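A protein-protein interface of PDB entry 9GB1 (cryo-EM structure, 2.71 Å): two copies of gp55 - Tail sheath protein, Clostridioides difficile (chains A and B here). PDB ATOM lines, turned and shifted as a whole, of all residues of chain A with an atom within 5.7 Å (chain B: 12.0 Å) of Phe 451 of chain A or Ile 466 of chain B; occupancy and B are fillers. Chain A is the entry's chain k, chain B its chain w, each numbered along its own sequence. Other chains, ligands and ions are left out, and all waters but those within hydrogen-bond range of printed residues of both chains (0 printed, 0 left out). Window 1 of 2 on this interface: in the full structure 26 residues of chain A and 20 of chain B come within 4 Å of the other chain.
The side-chain amide nitrogen of Gln 411 of chain A sits at hydrogen-bond distance from the side-chain amide oxygen of Asn 406 of chain A.
O of Asp 449 of chain A sits at hydrogen-bond distance from ND2 of Asn 406 of chain A.
The backbone carbonyl oxygen of Glu 450 of chain A is in hydrogen-bond range of the side-chain amide nitrogen of Asn 406 of chain A.
NE2 of Gln 443 of chain A sits at hydrogen-bond distance from O of Glu 450 of chain A.
The side-chain amide oxygen (OE1) of Gln 443 of chain A lies within hydrogen-bond range of the backbone NH (N) of Tyr 452 of chain A, at 2.5 Å.
The side-chain amide nitrogen of Asn 322 of chain B sits at hydrogen-bond distance from the backbone carbonyl oxygen of Val 360 of chain B, at 2.9 Å.
Ile 466 of chain B touches Phe 400 of chain A (CD1 to CE2, 3.2 Å).
Val 401 of chain A touches Asn 322 of chain B.
Val 401 of chain A touches Met 463 of chain B.
CG2 of Val 401 of chain A touches CD1 of Ile 466 of chain B, 3.8 Å away.
OD1 of Asp 449 of chain A touches C of Met 463 of chain B, at 3.2 Å.
Lys 465 of chain B touches Glu 450 of chain A.
Met 463 of chain B touches Phe 451 of chain A.
O of Phe 451 of chain A touches CA of Ile 466 of chain B, 3.3 Å away.
Tyr 452 of chain A touches Tyr 467 of chain B (CE1 to CD2, 3.2 Å).
NE1 of Trp 453 of chain A touches CG2 of Ile 466 of chain B, at 3.7 Å.
Of chain B, only Asn 322, Met 463, Lys 464 and Ile 466 come within 4 Å of Val 401 of chain A.
Of chain B, only Asp 461 (3.2 Å) and Met 463 (3.8 Å) come within 4 Å of Asn 406 of chain A.
Gln 411 of chain A touches one residue of chain B.
No residue of chain B comes within 4 Å of Ile 438 of chain A.
Glu 450 of chain A touches two residues of chain B.
Of chain B, only Met 463, Lys 465, Ile 466 and Tyr 467 come within 4 Å of Phe 451 of chain A.
Of chain B, only Tyr 467 (3.2 Å) comes within 4 Å of Tyr 452 of chain A.
Of chain B, only Ile 466, Tyr 467, Gly 468 and Thr 469 come within 4 Å of Trp 453 of chain A.
Printed residues of chain A within 4 Å of Lys 464 of chain B: Val 401 (3.2 Å) and Asp 449 (2.5 Å).
Of chain A, only Phe 400 (3.2 Å), Val 401 (3.8 Å), Phe 451 (3.3 Å) and Trp 453 (3.7 Å) come within 4 Å of Ile 466 of chain B.
Printed residues of chain A within 4 Å of Tyr 467 of chain B: Glu 450, Phe 451, Tyr 452 and Trp 453.
The nearest residue of chain B that does not touch Phe 451 of chain A is Gly 468 of chain B (5.8 Å).
The nearest residue of chain A that does not touch Ile 466 of chain B is Glu 450 of chain A (5.0 Å).
No position is printed for both chains.
Of the 24 pairs that touch across the chains among the printed residues, none has its exchanged pair printed and touching as well.
The backbone NH (N) of Asn 406 of chain A sits at hydrogen-bond distance from the backbone carbonyl oxygen (O) of Asp 461 of chain B (3.2 Å).
OD1 of Asp 449 of chain A sits close to O of Val 462 of chain B, at 2.6 Å.
The side-chain carboxylate (OD1) of Asp 449 of chain A is in hydrogen-bond range of the backbone NH (N) of Lys 464 of chain B (2.5 Å).
The side-chain amino group (NZ) of Lys 465 of chain B is in salt-bridge range of the side-chain carboxylate (OD2) of Asp 449 of chain A (3.9 Å).
The side-chain carboxylate of Glu 450 of chain A sits at hydrogen-bond distance from the side-chain hydroxyl of Tyr 467 of chain B.
The backbone NH (N) of Phe 451 of chain A is in hydrogen-bond range of the backbone carbonyl oxygen (O) of Lys 465 of chain B, 3.1 Å away.
The backbone NH (N) of Tyr 467 of chain B sits at hydrogen-bond distance from the backbone carbonyl oxygen (O) of Phe 451 of chain A, at 3.2 Å.
O of Tyr 467 of chain B sits at hydrogen-bond distance from N of Trp 453 of chain A (3.1 Å).
O of Trp 453 of chain A lies within hydrogen-bond range of N of Thr 469 of chain B (3.1 Å).
Of the 15 printed residues of chain A, 10 touch a printed residue of chain B.
Hydrophobic or aromatic side chains of chain A that line the printed part of chain B: Phe 400, Val 401, Val 414, Phe 451, Tyr 452 and Trp 453.
Of the 14 printed residues of chain B, 10 touch a printed residue of chain A.
Among the printed residues, 24 pairs touch across the chains.
Among the printed residues, Asp or Glu carboxylates within 4 Å of a Lys or Arg side-chain nitrogen of the other chain: Asp 449 of chain A with Lys 465 of chain B (3.9 Å).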
ATOM      1  N   PHE A 400     -31.956   3.841 -27.266  1.00  0.00           N
ATOM      2  CA  PHE A 400     -30.555   3.836 -26.873  1.00  0.00           C
ATOM      3  C   PHE A 400     -29.707   4.812 -27.686  1.00  0.00           C
ATOM      4  O   PHE A 400     -28.772   5.414 -27.154  1.00  0.00           O
ATOM      5  CB  PHE A 400     -30.050   2.422 -27.065  1.00  0.00           C
ATOM      6  CG  PHE A 400     -28.641   2.200 -26.653  1.00  0.00           C
ATOM      7  CD1 PHE A 400     -28.313   2.089 -25.320  1.00  0.00           C
ATOM      8  CD2 PHE A 400     -27.636   2.127 -27.592  1.00  0.00           C
ATOM      9  CE1 PHE A 400     -27.027   1.859 -24.953  1.00  0.00           C
ATOM     10  CE2 PHE A 400     -26.363   1.901 -27.219  1.00  0.00           C
ATOM     11  CZ  PHE A 400     -26.056   1.768 -25.918  1.00  0.00           C
ATOM     12  N   VAL A 401     -30.011   4.955 -28.976  1.00  0.00           N
ATOM     13  CA  VAL A 401     -29.291   5.842 -29.888  1.00  0.00           C
ATOM     14  C   VAL A 401     -30.157   7.061 -30.156  1.00  0.00           C
ATOM     15  O   VAL A 401     -31.325   6.929 -30.544  1.00  0.00           O
ATOM     16  CB  VAL A 401     -28.918   5.140 -31.205  1.00  0.00           C
ATOM     17  CG1 VAL A 401     -28.275   6.129 -32.159  1.00  0.00           C
ATOM     18  CG2 VAL A 401     -27.951   4.007 -30.942  1.00  0.00           C
ATOM     19  N   ASN A 406     -23.788  11.176 -23.861  1.00  0.00           N
ATOM     20  CA  ASN A 406     -22.458  10.634 -24.134  1.00  0.00           C
ATOM     21  C   ASN A 406     -21.467  11.018 -23.040  1.00  0.00           C
ATOM     22  O   ASN A 406     -20.321  11.383 -23.314  1.00  0.00           O
ATOM     23  CB  ASN A 406     -21.948  11.098 -25.495  1.00  0.00           C
ATOM     24  CG  ASN A 406     -20.827  10.224 -26.026  1.00  0.00           C
ATOM     25  OD1 ASN A 406     -20.198   9.478 -25.278  1.00  0.00           O
ATOM     26  ND2 ASN A 406     -20.571  10.315 -27.324  1.00  0.00           N
ATOM     27  N   GLN A 411     -22.433   6.130 -20.748  1.00  0.00           N
ATOM     28  CA  GLN A 411     -21.563   5.036 -21.165  1.00  0.00           C
ATOM     29  C   GLN A 411     -21.625   3.877 -20.179  1.00  0.00           C
ATOM     30  O   GLN A 411     -21.602   2.707 -20.577  1.00  0.00           O
ATOM     31  CB  GLN A 411     -20.126   5.535 -21.309  1.00  0.00           C
ATOM     32  CG  GLN A 411     -19.924   6.575 -22.394  1.00  0.00           C
ATOM     33  CD  GLN A 411     -18.514   7.128 -22.409  1.00  0.00           C
ATOM     34  OE1 GLN A 411     -17.697   6.799 -21.548  1.00  0.00           O
ATOM     35  NE2 GLN A 411     -18.219   7.969 -23.390  1.00  0.00           N
ATOM     36  N   VAL A 414     -24.691   2.010 -20.789  1.00  0.00           N
ATOM     37  CA  VAL A 414     -24.506   1.208 -21.998  1.00  0.00           C
ATOM     38  C   VAL A 414     -23.810  -0.099 -21.655  1.00  0.00           C
ATOM     39  O   VAL A 414     -24.248  -1.190 -22.050  1.00  0.00           O
ATOM     40  CB  VAL A 414     -23.682   1.987 -23.038  1.00  0.00           C
ATOM     41  CG1 VAL A 414     -23.274   1.053 -24.188  1.00  0.00           C
ATOM     42  CG2 VAL A 414     -24.397   3.261 -23.492  1.00  0.00           C
ATOM     43  N   ILE A 415     -22.693   0.004 -20.939  1.00  0.00           N
ATOM     44  CA  ILE A 415     -21.916  -1.179 -20.599  1.00  0.00           C
ATOM     45  C   ILE A 415     -22.717  -2.089 -19.683  1.00  0.00           C
ATOM     46  O   ILE A 415     -22.627  -3.316 -19.776  1.00  0.00           O
ATOM     47  CB  ILE A 415     -20.565  -0.778 -19.975  1.00  0.00           C
ATOM     48  CG1 ILE A 415     -19.718   0.047 -20.959  1.00  0.00           C
ATOM     49  CG2 ILE A 415     -19.809  -2.002 -19.505  1.00  0.00           C
ATOM     50  CD1 ILE A 415     -19.196  -0.705 -22.179  1.00  0.00           C
ATOM     51  N   ILE A 438     -14.983  -0.520 -21.917  1.00  0.00           N
ATOM     52  CA  ILE A 438     -14.771   0.589 -22.839  1.00  0.00           C
ATOM     53  C   ILE A 438     -13.507   0.324 -23.642  1.00  0.00           C
ATOM     54  O   ILE A 438     -12.522  -0.208 -23.117  1.00  0.00           O
ATOM     55  CB  ILE A 438     -14.661   1.926 -22.077  1.00  0.00           C
ATOM     56  CG1 ILE A 438     -15.840   2.160 -21.119  1.00  0.00           C
ATOM     57  CG2 ILE A 438     -14.553   3.085 -23.060  1.00  0.00           C
ATOM     58  CD1 ILE A 438     -17.117   2.537 -21.795  1.00  0.00           C
ATOM     59  N   GLN A 443     -11.192   5.109 -27.846  1.00  0.00           N
ATOM     60  CA  GLN A 443     -12.044   6.139 -27.253  1.00  0.00           C
ATOM     61  C   GLN A 443     -11.266   7.410 -26.952  1.00  0.00           C
ATOM     62  O   GLN A 443     -11.852   8.497 -26.926  1.00  0.00           O
ATOM     63  CB  GLN A 443     -12.717   5.623 -25.980  1.00  0.00           C
ATOM     64  CG  GLN A 443     -13.875   6.494 -25.471  1.00  0.00           C
ATOM     65  CD  GLN A 443     -15.117   6.436 -26.340  1.00  0.00           C
ATOM     66  OE1 GLN A 443     -15.315   5.497 -27.101  1.00  0.00           O
ATOM     67  NE2 GLN A 443     -15.962   7.451 -26.226  1.00  0.00           N
ATOM     68  N   ALA A 446     -11.587   9.366 -29.943  1.00  0.00           N
ATOM     69  CA  ALA A 446     -12.956   9.441 -30.425  1.00  0.00           C
ATOM     70  C   ALA A 446     -13.407  10.882 -30.609  1.00  0.00           C
ATOM     71  O   ALA A 446     -12.934  11.803 -29.939  1.00  0.00           O
ATOM     72  CB  ALA A 446     -13.912   8.757 -29.453  1.00  0.00           C
ATOM     73  N   LYS A 447     -14.341  11.062 -31.534  1.00  0.00           N
ATOM     74  CA  LYS A 447     -15.107  12.290 -31.630  1.00  0.00           C
ATOM     75  C   LYS A 447     -16.162  12.303 -30.523  1.00  0.00           C
ATOM     76  O   LYS A 447     -16.466  11.275 -29.911  1.00  0.00           O
ATOM     77  CB  LYS A 447     -15.726  12.396 -33.028  1.00  0.00           C
ATOM     78  CG  LYS A 447     -16.721  13.525 -33.258  1.00  0.00           C
ATOM     79  CD  LYS A 447     -17.032  13.719 -34.733  1.00  0.00           C
ATOM     80  CE  LYS A 447     -18.094  12.733 -35.195  1.00  0.00           C
ATOM     81  NZ  LYS A 447     -19.474  13.246 -34.974  1.00  0.00           N
ATOM     82  N   ASP A 449     -19.373  12.587 -30.427  1.00  0.00           N
ATOM     83  CA  ASP A 449     -20.565  11.762 -30.592  1.00  0.00           C
ATOM     84  C   ASP A 449     -20.252  10.274 -30.522  1.00  0.00           C
ATOM     85  O   ASP A 449     -21.081   9.491 -30.044  1.00  0.00           O
ATOM     86  CB  ASP A 449     -21.234  12.089 -31.925  1.00  0.00           C
ATOM     87  CG  ASP A 449     -22.702  11.740 -31.940  1.00  0.00           C
ATOM     88  OD1 ASP A 449     -23.074  10.706 -31.346  1.00  0.00           O
ATOM     89  OD2 ASP A 449     -23.491  12.495 -32.546  1.00  0.00           O
ATOM     90  N   GLU A 450     -19.074   9.871 -30.981  1.00  0.00           N
ATOM     91  CA  GLU A 450     -18.740   8.458 -31.073  1.00  0.00           C
ATOM     92  C   GLU A 450     -18.559   7.854 -29.686  1.00  0.00           C
ATOM     93  O   GLU A 450     -18.008   8.487 -28.781  1.00  0.00           O
ATOM     94  CB  GLU A 450     -17.459   8.251 -31.891  1.00  0.00           C
ATOM     95  CG  GLU A 450     -17.288   9.068 -33.187  1.00  0.00           C
ATOM     96  CD  GLU A 450     -17.876   8.397 -34.406  1.00  0.00           C
ATOM     97  OE1 GLU A 450     -18.706   7.488 -34.248  1.00  0.00           O
ATOM     98  OE2 GLU A 450     -17.514   8.795 -35.534  1.00  0.00           O
ATOM     99  N   PHE A 451     -19.037   6.621 -29.526  1.00  0.00           N
ATOM    100  CA  PHE A 451     -18.772   5.797 -28.354  1.00  0.00           C
ATOM    101  C   PHE A 451     -18.187   4.474 -28.818  1.00  0.00           C
ATOM    102  O   PHE A 451     -18.728   3.852 -29.736  1.00  0.00           O
ATOM    103  CB  PHE A 451     -20.046   5.537 -27.546  1.00  0.00           C
ATOM    104  CG  PHE A 451     -19.825   4.695 -26.320  1.00  0.00           C
ATOM    105  CD1 PHE A 451     -18.714   4.879 -25.515  1.00  0.00           C
ATOM    106  CD2 PHE A 451     -20.703   3.681 -26.005  1.00  0.00           C
ATOM    107  CE1 PHE A 451     -18.512   4.096 -24.410  1.00  0.00           C
ATOM    108  CE2 PHE A 451     -20.495   2.898 -24.900  1.00  0.00           C
ATOM    109  CZ  PHE A 451     -19.404   3.103 -24.105  1.00  0.00           C
ATOM    110  N   TYR A 452     -17.098   4.037 -28.184  1.00  0.00           N
ATOM    111  CA  TYR A 452     -16.359   2.870 -28.647  1.00  0.00           C
ATOM    112  C   TYR A 452     -16.312   1.877 -27.496  1.00  0.00           C
ATOM    113  O   TYR A 452     -15.991   2.259 -26.367  1.00  0.00           O
ATOM    114  CB  TYR A 452     -14.925   3.221 -29.030  1.00  0.00           C
ATOM    115  CG  TYR A 452     -14.777   4.226 -30.147  1.00  0.00           C
ATOM    116  CD1 TYR A 452     -15.715   4.386 -31.138  1.00  0.00           C
ATOM    117  CD2 TYR A 452     -13.649   5.000 -30.207  1.00  0.00           C
ATOM    118  CE1 TYR A 452     -15.531   5.338 -32.120  1.00  0.00           C
ATOM    119  CE2 TYR A 452     -13.444   5.924 -31.200  1.00  0.00           C
ATOM    120  CZ  TYR A 452     -14.394   6.093 -32.159  1.00  0.00           C
ATOM    121  OH  TYR A 452     -14.219   7.020 -33.160  1.00  0.00           O
ATOM    122  N   TRP A 453     -16.620   0.614 -27.774  1.00  0.00           N
ATOM    123  CA  TRP A 453     -16.514  -0.437 -26.771  1.00  0.00           C
ATOM    124  C   TRP A 453     -15.971  -1.706 -27.411  1.00  0.00           C
ATOM    125  O   TRP A 453     -15.875  -1.826 -28.635  1.00  0.00           O
ATOM    126  CB  TRP A 453     -17.863  -0.708 -26.096  1.00  0.00           C
ATOM    127  CG  TRP A 453     -18.926  -1.189 -27.020  1.00  0.00           C
ATOM    128  CD1 TRP A 453     -19.602  -0.454 -27.945  1.00  0.00           C
ATOM    129  CD2 TRP A 453     -19.458  -2.514 -27.093  1.00  0.00           C
ATOM    130  NE1 TRP A 453     -20.515  -1.241 -28.601  1.00  0.00           N
ATOM    131  CE2 TRP A 453     -20.446  -2.511 -28.094  1.00  0.00           C
ATOM    132  CE3 TRP A 453     -19.192  -3.704 -26.413  1.00  0.00           C
ATOM    133  CZ2 TRP A 453     -21.168  -3.650 -28.430  1.00  0.00           C
ATOM    134  CZ3 TRP A 453     -19.909  -4.832 -26.749  1.00  0.00           C
ATOM    135  CH2 TRP A 453     -20.884  -4.798 -27.748  1.00  0.00           C
ATOM    136  N   CYS B 321     -33.784  11.803 -34.824  1.00  0.00           N
ATOM    137  CA  CYS B 321     -32.819  11.135 -35.690  1.00  0.00           C
ATOM    138  C   CYS B 321     -33.209   9.684 -35.935  1.00  0.00           C
ATOM    139  O   CYS B 321     -33.188   9.210 -37.076  1.00  0.00           O
ATOM    140  CB  CYS B 321     -31.420  11.216 -35.079  1.00  0.00           C
ATOM    141  SG  CYS B 321     -31.325  10.641 -33.373  1.00  0.00           S
ATOM    142  N   ASN B 322     -33.555   8.960 -34.873  1.00  0.00           N
ATOM    143  CA  ASN B 322     -33.994   7.571 -34.965  1.00  0.00           C
ATOM    144  C   ASN B 322     -35.182   7.340 -34.044  1.00  0.00           C
ATOM    145  O   ASN B 322     -35.250   6.337 -33.325  1.00  0.00           O
ATOM    146  CB  ASN B 322     -32.857   6.601 -34.626  1.00  0.00           C
ATOM    147  CG  ASN B 322     -31.684   6.640 -35.627  1.00  0.00           C
ATOM    148  OD1 ASN B 322     -30.576   6.238 -35.271  1.00  0.00           O
ATOM    149  ND2 ASN B 322     -31.922   7.061 -36.873  1.00  0.00           N
ATOM    150  N   GLN B 336     -26.526   1.539 -47.806  1.00  0.00           N
ATOM    151  CA  GLN B 336     -25.847   2.449 -46.884  1.00  0.00           C
ATOM    152  C   GLN B 336     -25.075   3.533 -47.623  1.00  0.00           C
ATOM    153  O   GLN B 336     -25.097   4.699 -47.219  1.00  0.00           O
ATOM    154  CB  GLN B 336     -24.898   1.696 -45.953  1.00  0.00           C
ATOM    155  CG  GLN B 336     -25.551   0.772 -44.948  1.00  0.00           C
ATOM    156  CD  GLN B 336     -24.518   0.066 -44.090  1.00  0.00           C
ATOM    157  OE1 GLN B 336     -23.315   0.214 -44.305  1.00  0.00           O
ATOM    158  NE2 GLN B 336     -24.980  -0.662 -43.083  1.00  0.00           N
ATOM    159  N   VAL B 360     -33.944   7.951 -40.226  1.00  0.00           N
ATOM    160  CA  VAL B 360     -32.528   7.673 -40.464  1.00  0.00           C
ATOM    161  C   VAL B 360     -31.633   8.659 -39.719  1.00  0.00           C
ATOM    162  O   VAL B 360     -30.633   8.258 -39.117  1.00  0.00           O
ATOM    163  CB  VAL B 360     -32.224   7.672 -41.979  1.00  0.00           C
ATOM    164  CG1 VAL B 360     -32.424   9.054 -42.615  1.00  0.00           C
ATOM    165  CG2 VAL B 360     -30.812   7.170 -42.237  1.00  0.00           C
ATOM    166  N   ASP B 461     -23.408  16.397 -25.667  1.00  0.00           N
ATOM    167  CA  ASP B 461     -23.294  15.413 -26.729  1.00  0.00           C
ATOM    168  C   ASP B 461     -24.310  14.293 -26.534  1.00  0.00           C
ATOM    169  O   ASP B 461     -24.620  13.892 -25.409  1.00  0.00           O
ATOM    170  CB  ASP B 461     -21.879  14.843 -26.760  1.00  0.00           C
ATOM    171  CG  ASP B 461     -20.820  15.923 -26.725  1.00  0.00           C
ATOM    172  OD1 ASP B 461     -21.085  17.034 -27.231  1.00  0.00           O
ATOM    173  OD2 ASP B 461     -19.728  15.669 -26.176  1.00  0.00           O
ATOM    174  N   VAL B 462     -24.827  13.794 -27.652  1.00  0.00           N
ATOM    175  CA  VAL B 462     -25.789  12.698 -27.682  1.00  0.00           C
ATOM    176  C   VAL B 462     -25.193  11.594 -28.540  1.00  0.00           C
ATOM    177  O   VAL B 462     -24.749  11.853 -29.663  1.00  0.00           O
ATOM    178  CB  VAL B 462     -27.150  13.155 -28.243  1.00  0.00           C
ATOM    179  CG1 VAL B 462     -28.116  11.981 -28.371  1.00  0.00           C
ATOM    180  CG2 VAL B 462     -27.743  14.244 -27.364  1.00  0.00           C
ATOM    181  N   MET B 463     -25.177  10.372 -28.011  1.00  0.00           N
ATOM    182  CA  MET B 463     -24.657   9.243 -28.771  1.00  0.00           C
ATOM    183  C   MET B 463     -25.473   9.030 -30.036  1.00  0.00           C
ATOM    184  O   MET B 463     -26.705   8.945 -29.989  1.00  0.00           O
ATOM    185  CB  MET B 463     -24.676   7.967 -27.931  1.00  0.00           C
ATOM    186  CG  MET B 463     -23.723   7.952 -26.755  1.00  0.00           C
ATOM    187  SD  MET B 463     -23.846   6.400 -25.844  1.00  0.00           S
ATOM    188  CE  MET B 463     -22.713   6.687 -24.489  1.00  0.00           C
ATOM    189  N   LYS B 464     -24.780   8.950 -31.167  1.00  0.00           N
ATOM    190  CA  LYS B 464     -25.369   8.569 -32.442  1.00  0.00           C
ATOM    191  C   LYS B 464     -24.683   7.367 -33.063  1.00  0.00           C
ATOM    192  O   LYS B 464     -25.364   6.463 -33.554  1.00  0.00           O
ATOM    193  CB  LYS B 464     -25.322   9.750 -33.427  1.00  0.00           C
ATOM    194  CG  LYS B 464     -26.408  10.799 -33.190  1.00  0.00           C
ATOM    195  CD  LYS B 464     -26.650  11.687 -34.414  1.00  0.00           C
ATOM    196  CE  LYS B 464     -28.036  12.329 -34.385  1.00  0.00           C
ATOM    197  NZ  LYS B 464     -28.452  12.846 -35.716  1.00  0.00           N
ATOM    198  N   LYS B 465     -23.353   7.321 -33.026  1.00  0.00           N
ATOM    199  CA  LYS B 465     -22.565   6.251 -33.622  1.00  0.00           C
ATOM    200  C   LYS B 465     -21.863   5.468 -32.524  1.00  0.00           C
ATOM    201  O   LYS B 465     -21.228   6.057 -31.642  1.00  0.00           O
ATOM    202  CB  LYS B 465     -21.523   6.798 -34.592  1.00  0.00           C
ATOM    203  CG  LYS B 465     -22.016   7.110 -35.997  1.00  0.00           C
ATOM    204  CD  LYS B 465     -22.874   8.367 -36.094  1.00  0.00           C
ATOM    205  CE  LYS B 465     -22.061   9.638 -35.860  1.00  0.00           C
ATOM    206  NZ  LYS B 465     -22.881  10.866 -36.015  1.00  0.00           N
ATOM    207  N   ILE B 466     -21.990   4.146 -32.578  1.00  0.00           N
ATOM    208  CA  ILE B 466     -21.464   3.240 -31.566  1.00  0.00           C
ATOM    209  C   ILE B 466     -20.809   2.079 -32.299  1.00  0.00           C
ATOM    210  O   ILE B 466     -21.450   1.447 -33.144  1.00  0.00           O
ATOM    211  CB  ILE B 466     -22.580   2.746 -30.622  1.00  0.00           C
ATOM    212  CG1 ILE B 466     -23.494   3.920 -30.223  1.00  0.00           C
ATOM    213  CG2 ILE B 466     -21.989   2.067 -29.391  1.00  0.00           C
ATOM    214  CD1 ILE B 466     -24.592   3.580 -29.309  1.00  0.00           C
ATOM    215  N   TYR B 467     -19.535   1.806 -32.003  1.00  0.00           N
ATOM    216  CA  TYR B 467     -18.803   0.752 -32.696  1.00  0.00           C
ATOM    217  C   TYR B 467     -18.333  -0.258 -31.657  1.00  0.00           C
ATOM    218  O   TYR B 467     -17.721   0.125 -30.653  1.00  0.00           O
ATOM    219  CB  TYR B 467     -17.600   1.288 -33.475  1.00  0.00           C
ATOM    220  CG  TYR B 467     -17.859   2.529 -34.296  1.00  0.00           C
ATOM    221  CD1 TYR B 467     -18.944   2.658 -35.135  1.00  0.00           C
ATOM    222  CD2 TYR B 467     -16.913   3.519 -34.334  1.00  0.00           C
ATOM    223  CE1 TYR B 467     -19.128   3.823 -35.878  1.00  0.00           C
ATOM    224  CE2 TYR B 467     -17.080   4.665 -35.079  1.00  0.00           C
ATOM    225  CZ  TYR B 467     -18.183   4.806 -35.858  1.00  0.00           C
ATOM    226  OH  TYR B 467     -18.352   5.943 -36.613  1.00  0.00           O
ATOM    227  N   GLY B 468     -18.606  -1.538 -31.906  1.00  0.00           N
ATOM    228  CA  GLY B 468     -18.176  -2.615 -31.031  1.00  0.00           C
ATOM    229  C   GLY B 468     -17.207  -3.564 -31.703  1.00  0.00           C
ATOM    230  O   GLY B 468     -17.509  -4.116 -32.765  1.00  0.00           O
ATOM    231  N   THR B 469     -16.041  -3.768 -31.092  1.00  0.00           N
ATOM    232  CA  THR B 469     -14.999  -4.636 -31.630  1.00  0.00           C
ATOM    233  C   THR B 469     -15.077  -5.982 -30.919  1.00  0.00           C
ATOM    234  O   THR B 469     -14.789  -6.078 -29.722  1.00  0.00           O
ATOM    235  CB  THR B 469     -13.617  -4.010 -31.454  1.00  0.00           C
ATOM    236  OG1 THR B 469     -13.344  -3.826 -30.060  1.00  0.00           O
ATOM    237  CG2 THR B 469     -13.535  -2.670 -32.169  1.00  0.00           C
ATOM    238  N   GLY B 470     -15.461  -7.022 -31.664  1.00  0.00           N
ATOM    239  CA  GLY B 470     -15.627  -8.337 -31.089  1.00  0.00           C
ATOM    240  C   GLY B 470     -14.368  -9.183 -31.140  1.00  0.00           C
ATOM    241  O   GLY B 470     -13.469  -8.964 -31.949  1.00  0.00           O
